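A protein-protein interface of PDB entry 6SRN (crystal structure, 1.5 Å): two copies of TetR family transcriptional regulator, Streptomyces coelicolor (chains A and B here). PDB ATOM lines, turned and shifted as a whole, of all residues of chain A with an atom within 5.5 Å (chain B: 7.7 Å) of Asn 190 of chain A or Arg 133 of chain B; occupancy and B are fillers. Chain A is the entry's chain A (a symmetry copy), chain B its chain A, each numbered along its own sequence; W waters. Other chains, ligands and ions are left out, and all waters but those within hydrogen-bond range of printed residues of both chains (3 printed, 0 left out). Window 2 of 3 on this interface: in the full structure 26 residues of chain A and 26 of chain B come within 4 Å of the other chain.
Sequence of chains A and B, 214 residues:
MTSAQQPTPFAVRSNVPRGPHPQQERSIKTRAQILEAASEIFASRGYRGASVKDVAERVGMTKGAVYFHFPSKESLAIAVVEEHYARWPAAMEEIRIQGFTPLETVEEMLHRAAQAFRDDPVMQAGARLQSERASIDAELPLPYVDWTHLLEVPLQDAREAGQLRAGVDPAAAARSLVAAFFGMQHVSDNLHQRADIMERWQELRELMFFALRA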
ATOM      1  N   GLN A 185      18.149  -6.828 -14.230  1.00  0.00           N
ATOM      2  CA  GLN A 185      17.228  -5.696 -14.054  1.00  0.00           C
ATOM      3  C   GLN A 185      17.864  -4.624 -13.168  1.00  0.00           C
ATOM      4  O   GLN A 185      17.604  -3.450 -13.345  1.00  0.00           O
ATOM      5  CB  GLN A 185      15.851  -6.148 -13.605  1.00  0.00           C
ATOM      6  CG  GLN A 185      15.762  -6.688 -12.172  1.00  0.00           C
ATOM      7  CD  GLN A 185      15.724  -5.568 -11.144  1.00  0.00           C
ATOM      8  OE1 GLN A 185      15.184  -4.500 -11.366  1.00  0.00           O
ATOM      9  NE2 GLN A 185      16.298  -5.826  -9.989  1.00  0.00           N
ATOM     10  N   HIS A 186      18.667  -5.049 -12.189  1.00  0.00           N
ATOM     11  CA  HIS A 186      19.339  -4.126 -11.290  1.00  0.00           C
ATOM     12  C   HIS A 186      20.368  -3.296 -12.021  1.00  0.00           C
ATOM     13  O   HIS A 186      20.445  -2.089 -11.826  1.00  0.00           O
ATOM     14  CB  HIS A 186      19.957  -4.891 -10.137  1.00  0.00           C
ATOM     15  CG  HIS A 186      20.370  -4.020  -9.032  1.00  0.00           C
ATOM     16  ND1 HIS A 186      19.476  -3.518  -8.112  1.00  0.00           N
ATOM     17  CD2 HIS A 186      21.587  -3.555  -8.673  1.00  0.00           C
ATOM     18  CE1 HIS A 186      20.131  -2.758  -7.253  1.00  0.00           C
ATOM     19  NE2 HIS A 186      21.414  -2.807  -7.548  1.00  0.00           N
ATOM     20  N   VAL A 187      21.167  -3.960 -12.867  1.00  0.00           N
ATOM     21  CA  VAL A 187      22.113  -3.212 -13.647  1.00  0.00           C
ATOM     22  C   VAL A 187      21.399  -2.196 -14.539  1.00  0.00           C
ATOM     23  O   VAL A 187      21.838  -1.057 -14.663  1.00  0.00           O
ATOM     24  CB  VAL A 187      23.013  -4.151 -14.515  1.00  0.00           C
ATOM     25  CG1 VAL A 187      23.811  -3.376 -15.571  1.00  0.00           C
ATOM     26  CG2 VAL A 187      23.911  -5.046 -13.660  1.00  0.00           C
ATOM     27  N   SER A 188      20.336  -2.639 -15.187  1.00  0.00           N
ATOM     28  CA  SER A 188      19.553  -1.772 -16.041  1.00  0.00           C
ATOM     29  C   SER A 188      18.981  -0.583 -15.273  1.00  0.00           C
ATOM     30  O   SER A 188      19.012   0.549 -15.758  1.00  0.00           O
ATOM     31  CB  SER A 188      18.446  -2.577 -16.721  1.00  0.00           C
ATOM     32  OG  SER A 188      17.686  -1.785 -17.629  1.00  0.00           O
ATOM     33  N   ASP A 189      18.504  -0.799 -14.055  1.00  0.00           N
ATOM     34  CA  ASP A 189      18.011   0.273 -13.237  1.00  0.00           C
ATOM     35  C   ASP A 189      19.147   1.234 -12.889  1.00  0.00           C
ATOM     36  O   ASP A 189      19.017   2.443 -13.038  1.00  0.00           O
ATOM     37  CB  ASP A 189      17.406  -0.303 -11.936  1.00  0.00           C
ATOM     38  CG  ASP A 189      17.347   0.710 -10.774  1.00  0.00           C
ATOM     39  OD1 ASP A 189      18.325   0.940  -9.989  1.00  0.00           O
ATOM     40  OD2 ASP A 189      16.307   1.261 -10.653  1.00  0.00           O
ATOM     41  N   ASN A 190      20.248   0.688 -12.381  1.00  0.00           N
ATOM     42  CA  ASN A 190      21.312   1.520 -11.845  1.00  0.00           C
ATOM     43  C   ASN A 190      21.897   2.409 -12.928  1.00  0.00           C
ATOM     44  O   ASN A 190      22.164   3.603 -12.665  1.00  0.00           O
ATOM     45  CB  ASN A 190      22.455   0.680 -11.281  1.00  0.00           C
ATOM     46  CG  ASN A 190      22.160   0.017  -9.936  1.00  0.00           C
ATOM     47  OD1 ASN A 190      23.089  -0.529  -9.358  1.00  0.00           O
ATOM     48  ND2 ASN A 190      20.947   0.079  -9.417  1.00  0.00           N
ATOM     49  N   LEU A 191      22.161   1.820 -14.106  1.00  0.00           N
ATOM     50  CA  LEU A 191      22.821   2.549 -15.161  1.00  0.00           C
ATOM     51  C   LEU A 191      21.901   3.352 -16.040  1.00  0.00           C
ATOM     52  O   LEU A 191      22.274   4.449 -16.466  1.00  0.00           O
ATOM     53  CB  LEU A 191      23.641   1.605 -16.043  1.00  0.00           C
ATOM     54  CG  LEU A 191      24.783   0.837 -15.334  1.00  0.00           C
ATOM     55  CD1 LEU A 191      25.511  -0.032 -16.367  1.00  0.00           C
ATOM     56  CD2 LEU A 191      25.731   1.782 -14.624  1.00  0.00           C
ATOM     57  N   HIS A 192      20.705   2.815 -16.296  1.00  0.00           N
ATOM     58  CA  HIS A 192      19.839   3.346 -17.339  1.00  0.00           C
ATOM     59  C   HIS A 192      18.389   3.510 -16.970  1.00  0.00           C
ATOM     60  O   HIS A 192      17.541   3.737 -17.860  1.00  0.00           O
ATOM     61  CB  HIS A 192      19.955   2.468 -18.596  1.00  0.00           C
ATOM     62  CG  HIS A 192      21.356   2.306 -19.092  1.00  0.00           C
ATOM     63  ND1 HIS A 192      22.133   3.368 -19.507  1.00  0.00           N
ATOM     64  CD2 HIS A 192      22.133   1.208 -19.215  1.00  0.00           C
ATOM     65  CE1 HIS A 192      23.334   2.938 -19.848  1.00  0.00           C
ATOM     66  NE2 HIS A 192      23.359   1.632 -19.683  1.00  0.00           N
ATOM     67  N   GLN A 193      18.068   3.446 -15.689  1.00  0.00           N
ATOM     68  CA  GLN A 193      16.708   3.606 -15.205  1.00  0.00           C
ATOM     69  C   GLN A 193      15.713   2.632 -15.903  1.00  0.00           C
ATOM     70  O   GLN A 193      14.565   2.975 -16.203  1.00  0.00           O
ATOM     71  CB  GLN A 193      16.219   5.066 -15.349  1.00  0.00           C
ATOM     72  CG  GLN A 193      17.018   6.068 -14.526  1.00  0.00           C
ATOM     73  CD  GLN A 193      18.469   6.242 -14.975  1.00  0.00           C
ATOM     74  OE1 GLN A 193      19.397   5.913 -14.228  1.00  0.00           O
ATOM     75  NE2 GLN A 193      18.679   6.771 -16.204  1.00  0.00           N
ATOM     76  N   ALA B 127      31.233  -3.767  -2.865  1.00  0.00           N
ATOM     77  CA  ALA B 127      29.883  -4.154  -3.233  1.00  0.00           C
ATOM     78  C   ALA B 127      28.845  -3.493  -2.340  1.00  0.00           C
ATOM     79  O   ALA B 127      27.819  -2.956  -2.814  1.00  0.00           O
ATOM     80  CB  ALA B 127      29.699  -5.679  -3.231  1.00  0.00           C
ATOM     81  N   ARG B 128      29.084  -3.461  -1.029  1.00  0.00           N
ATOM     82  CA  ARG B 128      28.107  -2.848  -0.161  1.00  0.00           C
ATOM     83  C   ARG B 128      27.972  -1.369  -0.416  1.00  0.00           C
ATOM     84  O   ARG B 128      26.853  -0.845  -0.427  1.00  0.00           O
ATOM     85  CB  ARG B 128      28.438  -3.096   1.313  1.00  0.00           C
ATOM     86  CG  ARG B 128      27.379  -2.516   2.240  1.00  0.00           C
ATOM     87  CD  ARG B 128      27.405  -3.147   3.605  1.00  0.00           C
ATOM     88  NE  ARG B 128      26.313  -2.597   4.424  1.00  0.00           N
ATOM     89  CZ  ARG B 128      26.009  -3.038   5.648  1.00  0.00           C
ATOM     90  NH1 ARG B 128      26.717  -3.989   6.204  1.00  0.00           N
ATOM     91  NH2 ARG B 128      24.972  -2.514   6.313  1.00  0.00           N
ATOM     92  N   LEU B 129      29.085  -0.663  -0.606  1.00  0.00           N
ATOM     93  CA  LEU B 129      29.010   0.771  -0.920  1.00  0.00           C
ATOM     94  C   LEU B 129      28.242   1.014  -2.224  1.00  0.00           C
ATOM     95  O   LEU B 129      27.389   1.925  -2.278  1.00  0.00           O
ATOM     96  CB  LEU B 129      30.410   1.351  -0.962  1.00  0.00           C
ATOM     97  CG  LEU B 129      31.151   1.334   0.376  1.00  0.00           C
ATOM     98  CD1 LEU B 129      32.628   1.602   0.180  1.00  0.00           C
ATOM     99  CD2 LEU B 129      30.555   2.334   1.334  1.00  0.00           C
ATOM    100  N   GLN B 130      28.500   0.215  -3.251  1.00  0.00           N
ATOM    101  CA  GLN B 130      27.731   0.323  -4.521  1.00  0.00           C
ATOM    102  C   GLN B 130      26.246  -0.047  -4.349  1.00  0.00           C
ATOM    103  O   GLN B 130      25.369   0.488  -5.060  1.00  0.00           O
ATOM    104  CB  GLN B 130      28.320  -0.534  -5.611  1.00  0.00           C
ATOM    105  CG  GLN B 130      29.687  -0.104  -6.072  1.00  0.00           C
ATOM    106  CD  GLN B 130      29.671   1.175  -6.876  1.00  0.00           C
ATOM    107  OE1 GLN B 130      29.095   2.178  -6.446  1.00  0.00           O
ATOM    108  NE2 GLN B 130      30.326   1.161  -8.002  1.00  0.00           N
ATOM    109  N   SER B 131      25.947  -0.952  -3.422  1.00  0.00           N
ATOM    110  CA  SER B 131      24.546  -1.326  -3.162  1.00  0.00           C
ATOM    111  C   SER B 131      23.782  -0.158  -2.624  1.00  0.00           C
ATOM    112  O   SER B 131      22.556  -0.049  -2.849  1.00  0.00           O
ATOM    113  CB  SER B 131      24.434  -2.457  -2.119  1.00  0.00           C
ATOM    114  OG  SER B 131      24.353  -1.910  -0.789  1.00  0.00           O
ATOM    115  N   GLU B 132      24.484   0.684  -1.857  1.00  0.00           N
ATOM    116  CA  GLU B 132      23.989   1.817  -1.151  1.00  0.00           C
ATOM    117  C   GLU B 132      24.106   3.078  -1.990  1.00  0.00           C
ATOM    118  O   GLU B 132      23.775   4.122  -1.530  1.00  0.00           O
ATOM    119  CB  GLU B 132      24.718   1.985   0.201  1.00  0.00           C
ATOM    120  CG  GLU B 132      24.596   0.684   1.016  1.00  0.00           C
ATOM    121  CD  GLU B 132      25.080   0.710   2.444  1.00  0.00           C
ATOM    122  OE1 GLU B 132      25.769   1.695   2.802  1.00  0.00           O
ATOM    123  OE2 GLU B 132      24.782  -0.311   3.182  1.00  0.00           O
ATOM    124  N   ARG B 133      24.502   2.974  -3.259  1.00  0.00           N
ATOM    125  CA  ARG B 133      24.844   4.192  -4.009  1.00  0.00           C
ATOM    126  C   ARG B 133      23.745   5.249  -4.104  1.00  0.00           C
ATOM    127  O   ARG B 133      24.059   6.409  -4.147  1.00  0.00           O
ATOM    128  CB  ARG B 133      25.328   3.909  -5.432  1.00  0.00           C
ATOM    129  CG  ARG B 133      24.273   3.259  -6.319  1.00  0.00           C
ATOM    130  CD  ARG B 133      24.866   2.593  -7.540  1.00  0.00           C
ATOM    131  NE  ARG B 133      25.460   3.526  -8.487  1.00  0.00           N
ATOM    132  CZ  ARG B 133      24.878   4.035  -9.575  1.00  0.00           C
ATOM    133  NH1 ARG B 133      23.610   3.754  -9.919  1.00  0.00           N
ATOM    134  NH2 ARG B 133      25.584   4.812 -10.361  1.00  0.00           N
ATOM    135  N   ALA B 134      22.476   4.833  -4.188  1.00  0.00           N
ATOM    136  CA  ALA B 134      21.346   5.768  -4.296  1.00  0.00           C
ATOM    137  C   ALA B 134      21.176   6.658  -3.067  1.00  0.00           C
ATOM    138  O   ALA B 134      20.533   7.707  -3.146  1.00  0.00           O
ATOM    139  CB  ALA B 134      20.066   4.978  -4.533  1.00  0.00           C
ATOM    140  N   SER B 135      21.687   6.211  -1.916  1.00  0.00           N
ATOM    141  CA  SER B 135      21.662   7.016  -0.695  1.00  0.00           C
ATOM    142  C   SER B 135      23.031   7.208  -0.018  1.00  0.00           C
ATOM    143  O   SER B 135      23.119   7.304   1.202  1.00  0.00           O
ATOM    144  CB  SER B 135      20.683   6.394   0.312  1.00  0.00           C
ATOM    145  OG  SER B 135      20.924   5.014   0.472  1.00  0.00           O
ATOM    146  N   ILE B 136      24.090   7.223  -0.810  1.00  0.00           N
ATOM    147  CA  ILE B 136      25.401   7.690  -0.376  1.00  0.00           C
ATOM    148  C   ILE B 136      25.652   8.945  -1.191  1.00  0.00           C
ATOM    149  O   ILE B 136      25.701   8.898  -2.435  1.00  0.00           O
ATOM    150  CB  ILE B 136      26.532   6.645  -0.645  1.00  0.00           C
ATOM    151  CG1 ILE B 136      26.308   5.391   0.216  1.00  0.00           C
ATOM    152  CG2 ILE B 136      27.926   7.269  -0.415  1.00  0.00           C
ATOM    153  CD1 ILE B 136      27.317   4.282  -0.020  1.00  0.00           C
ATOM    154  N   ASP B 137      25.783  10.072  -0.506  1.00  0.00           N
ATOM    155  CA  ASP B 137      26.150  11.302  -1.163  1.00  0.00           C
ATOM    156  C   ASP B 137      27.672  11.270  -1.319  1.00  0.00           C
ATOM    157  O   ASP B 137      28.416  11.861  -0.536  1.00  0.00           O
ATOM    158  CB  ASP B 137      25.673  12.511  -0.337  1.00  0.00           C
ATOM    159  CG  ASP B 137      25.933  13.831  -1.021  1.00  0.00           C
ATOM    160  OD1 ASP B 137      25.758  13.924  -2.256  1.00  0.00           O
ATOM    161  OD2 ASP B 137      26.306  14.784  -0.314  1.00  0.00           O
ATOM    162  N   ALA B 138      28.118  10.539  -2.325  1.00  0.00           N
ATOM    163  CA  ALA B 138      29.546  10.558  -2.748  1.00  0.00           C
ATOM    164  C   ALA B 138      29.614  10.203  -4.241  1.00  0.00           C
ATOM    165  O   ALA B 138      28.809   9.421  -4.688  1.00  0.00           O
ATOM    166  CB  ALA B 138      30.369   9.569  -1.926  1.00  0.00           C
ATOM    167  N   LEU B 140      30.733   7.882  -6.388  1.00  0.00           N
ATOM    168  CA  LEU B 140      31.418   6.609  -6.546  1.00  0.00           C
ATOM    169  C   LEU B 140      31.501   6.264  -8.017  1.00  0.00           C
ATOM    170  O   LEU B 140      30.675   6.747  -8.817  1.00  0.00           O
ATOM    171  CB  LEU B 140      30.666   5.492  -5.791  1.00  0.00           C
ATOM    172  CG  LEU B 140      30.375   5.632  -4.316  1.00  0.00           C
ATOM    173  CD1 LEU B 140      29.584   4.411  -3.862  1.00  0.00           C
ATOM    174  CD2 LEU B 140      31.612   5.781  -3.435  1.00  0.00           C
ATOM    175  N   PRO B 141      32.490   5.466  -8.418  1.00  0.00           N
ATOM    176  CA  PRO B 141      32.594   4.992  -9.821  1.00  0.00           C
ATOM    177  C   PRO B 141      31.277   4.310 -10.269  1.00  0.00           C
ATOM    178  O   PRO B 141      30.595   3.640  -9.492  1.00  0.00           O
ATOM    179  CB  PRO B 141      33.777   4.046  -9.805  1.00  0.00           C
ATOM    180  CG  PRO B 141      34.518   4.261  -8.516  1.00  0.00           C
ATOM    181  CD  PRO B 141      33.508   4.840  -7.552  1.00  0.00           C
ATOM    182  N   LEU B 142      30.959   4.435 -11.551  1.00  0.00           N
ATOM    183  CA  LEU B 142      29.820   3.688 -12.079  1.00  0.00           C
ATOM    184  C   LEU B 142      30.063   2.195 -11.857  1.00  0.00           C
ATOM    185  O   LEU B 142      31.165   1.696 -12.177  1.00  0.00           O
ATOM    186  CB  LEU B 142      29.642   3.942 -13.579  1.00  0.00           C
ATOM    187  CG  LEU B 142      28.926   5.246 -13.980  1.00  0.00           C
ATOM    188  CD1 LEU B 142      29.035   5.393 -15.484  1.00  0.00           C
ATOM    189  CD2 LEU B 142      27.471   5.346 -13.572  1.00  0.00           C
ATOM    190  N   PRO B 143      29.036   1.494 -11.357  1.00  0.00           N
ATOM    191  CA  PRO B 143      29.160   0.024 -11.308  1.00  0.00           C
ATOM    192  C   PRO B 143      29.115  -0.655 -12.674  1.00  0.00           C
ATOM    193  O   PRO B 143      28.692  -0.048 -13.693  1.00  0.00           O
ATOM    194  CB  PRO B 143      27.973  -0.376 -10.456  1.00  0.00           C
ATOM    195  CG  PRO B 143      26.932   0.658 -10.812  1.00  0.00           C
ATOM    196  CD  PRO B 143      27.705   1.926 -10.893  1.00  0.00           C
ATOM    197  N   TYR B 144      29.596  -1.878 -12.708  1.00  0.00           N
ATOM    198  CA  TYR B 144      29.422  -2.862 -13.810  1.00  0.00           C
ATOM    199  C   TYR B 144      30.290  -2.589 -15.034  1.00  0.00           C
ATOM    200  O   TYR B 144      30.732  -3.551 -15.709  1.00  0.00           O
ATOM    201  CB  TYR B 144      27.932  -3.009 -14.236  1.00  0.00           C
ATOM    202  CG  TYR B 144      26.999  -3.063 -13.041  1.00  0.00           C
ATOM    203  CD1 TYR B 144      27.138  -4.032 -12.032  1.00  0.00           C
ATOM    204  CD2 TYR B 144      26.009  -2.095 -12.859  1.00  0.00           C
ATOM    205  CE1 TYR B 144      26.337  -4.007 -10.923  1.00  0.00           C
ATOM    206  CE2 TYR B 144      25.198  -2.095 -11.750  1.00  0.00           C
ATOM    207  CZ  TYR B 144      25.384  -3.032 -10.764  1.00  0.00           C
ATOM    208  OH  TYR B 144      24.604  -2.975  -9.643  1.00  0.00           O
ATOM    209  N   PHE B 182      26.834 -10.570 -10.968  1.00  0.00           N
ATOM    210  CA  PHE B 182      26.430  -9.603  -9.987  1.00  0.00           C
ATOM    211  C   PHE B 182      25.200 -10.084  -9.199  1.00  0.00           C
ATOM    212  O   PHE B 182      25.119 -10.007  -7.977  1.00  0.00           O
ATOM    213  CB  PHE B 182      26.108  -8.245 -10.618  1.00  0.00           C
ATOM    214  CG  PHE B 182      25.412  -7.370  -9.629  1.00  0.00           C
ATOM    215  CD1 PHE B 182      26.082  -6.793  -8.564  1.00  0.00           C
ATOM    216  CD2 PHE B 182      24.026  -7.226  -9.682  1.00  0.00           C
ATOM    217  CE1 PHE B 182      25.378  -6.110  -7.577  1.00  0.00           C
ATOM    218  CE2 PHE B 182      23.342  -6.541  -8.721  1.00  0.00           C
ATOM    219  CZ  PHE B 182      24.011  -5.970  -7.639  1.00  0.00           C
HETATM  220  O   HOH W   1      23.330  -0.666  -6.656  1.00  0.00           O
HETATM  221  O   HOH W   2      21.381   3.150  -8.135  1.00  0.00           O
HETATM  222  O   HOH W   3      23.903   6.328 -12.167  1.00  0.00           O
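The side-chain hydroxyl (OH) of Tyr 144 of chain B is in hydrogen-bond range of the side-chain amide oxygen (OD1) of Asn 190 of chain A (2.9 Å). The backbone carbonyl oxygen (O) of Asn 190 of chain A lies within hydrogen-bond range of the guanidinium group (NH1) of Arg 133 of chain B.
No position is printed for both chains.
ND2 of Asn 190 of chain A is in hydrogen-bond range of OD1 of Asp 189 of chain A. The side-chain amide nitrogen (ND2) of Asn 190 of chain A lies within hydrogen-bond range of the backbone carbonyl oxygen (O) of His 186 of chain A.
Along chain A the printed residues that touch a printed residue of chain B span positions 186 to 191. Hydrophobic or aromatic side chains of chain B within 4 Å of the printed part of chain A: Tyr 144 and Phe 182. Among the printed residues, 6 pairs touch across the chains. Among the printed residues, no Asp or Glu carboxylate lies within 4 Å of a Lys or Arg side-chain nitrogen of the other chain.
Printed residues of chain B within 4 Å of Val 187 of chain A: Tyr 144 (3.7 Å). Printed residues of chain B within 4 Å of Leu 191 of chain A: Pro 143. Arg 133 of chain B touches just one residue of chain A: Asn 190. The nearest printed residue of chain A that does not touch Tyr 144 of chain B is Leu 191 of chain A (4.03 Å).
Water W1 lies within hydrogen-bond range of the side-chain amide oxygen (OD1) of Asn 190 of chain A (2.7 Å), the backbone carbonyl oxygen (O) of Gln 130 of chain B (2.8 Å) and a ring nitrogen (NE2) of His 186 of chain A (3.0 Å). Water W3 lies within hydrogen-bond range of the guanidinium group of Arg 133 of chain B and the backbone carbonyl oxygen of Asn 190 of chain A. Water W2 bridges the guanidinium group of Arg 133 of chain B (2.9 Å) and the side-chain amide nitrogen of Asn 190 of chain A (3.4 Å).
CD2 of His 186 of chain A touches OH of Tyr 144 of chain B, at 3.2 Å. His 186 of chain A touches Phe 182 of chain B. CD2 of Tyr 144 of chain B touches CG2 of Val 187 of chain A, 3.7 Å away. CD2 of Leu 191 of chain A touches O of Pro 143 of chain B, at 3.6 Å.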
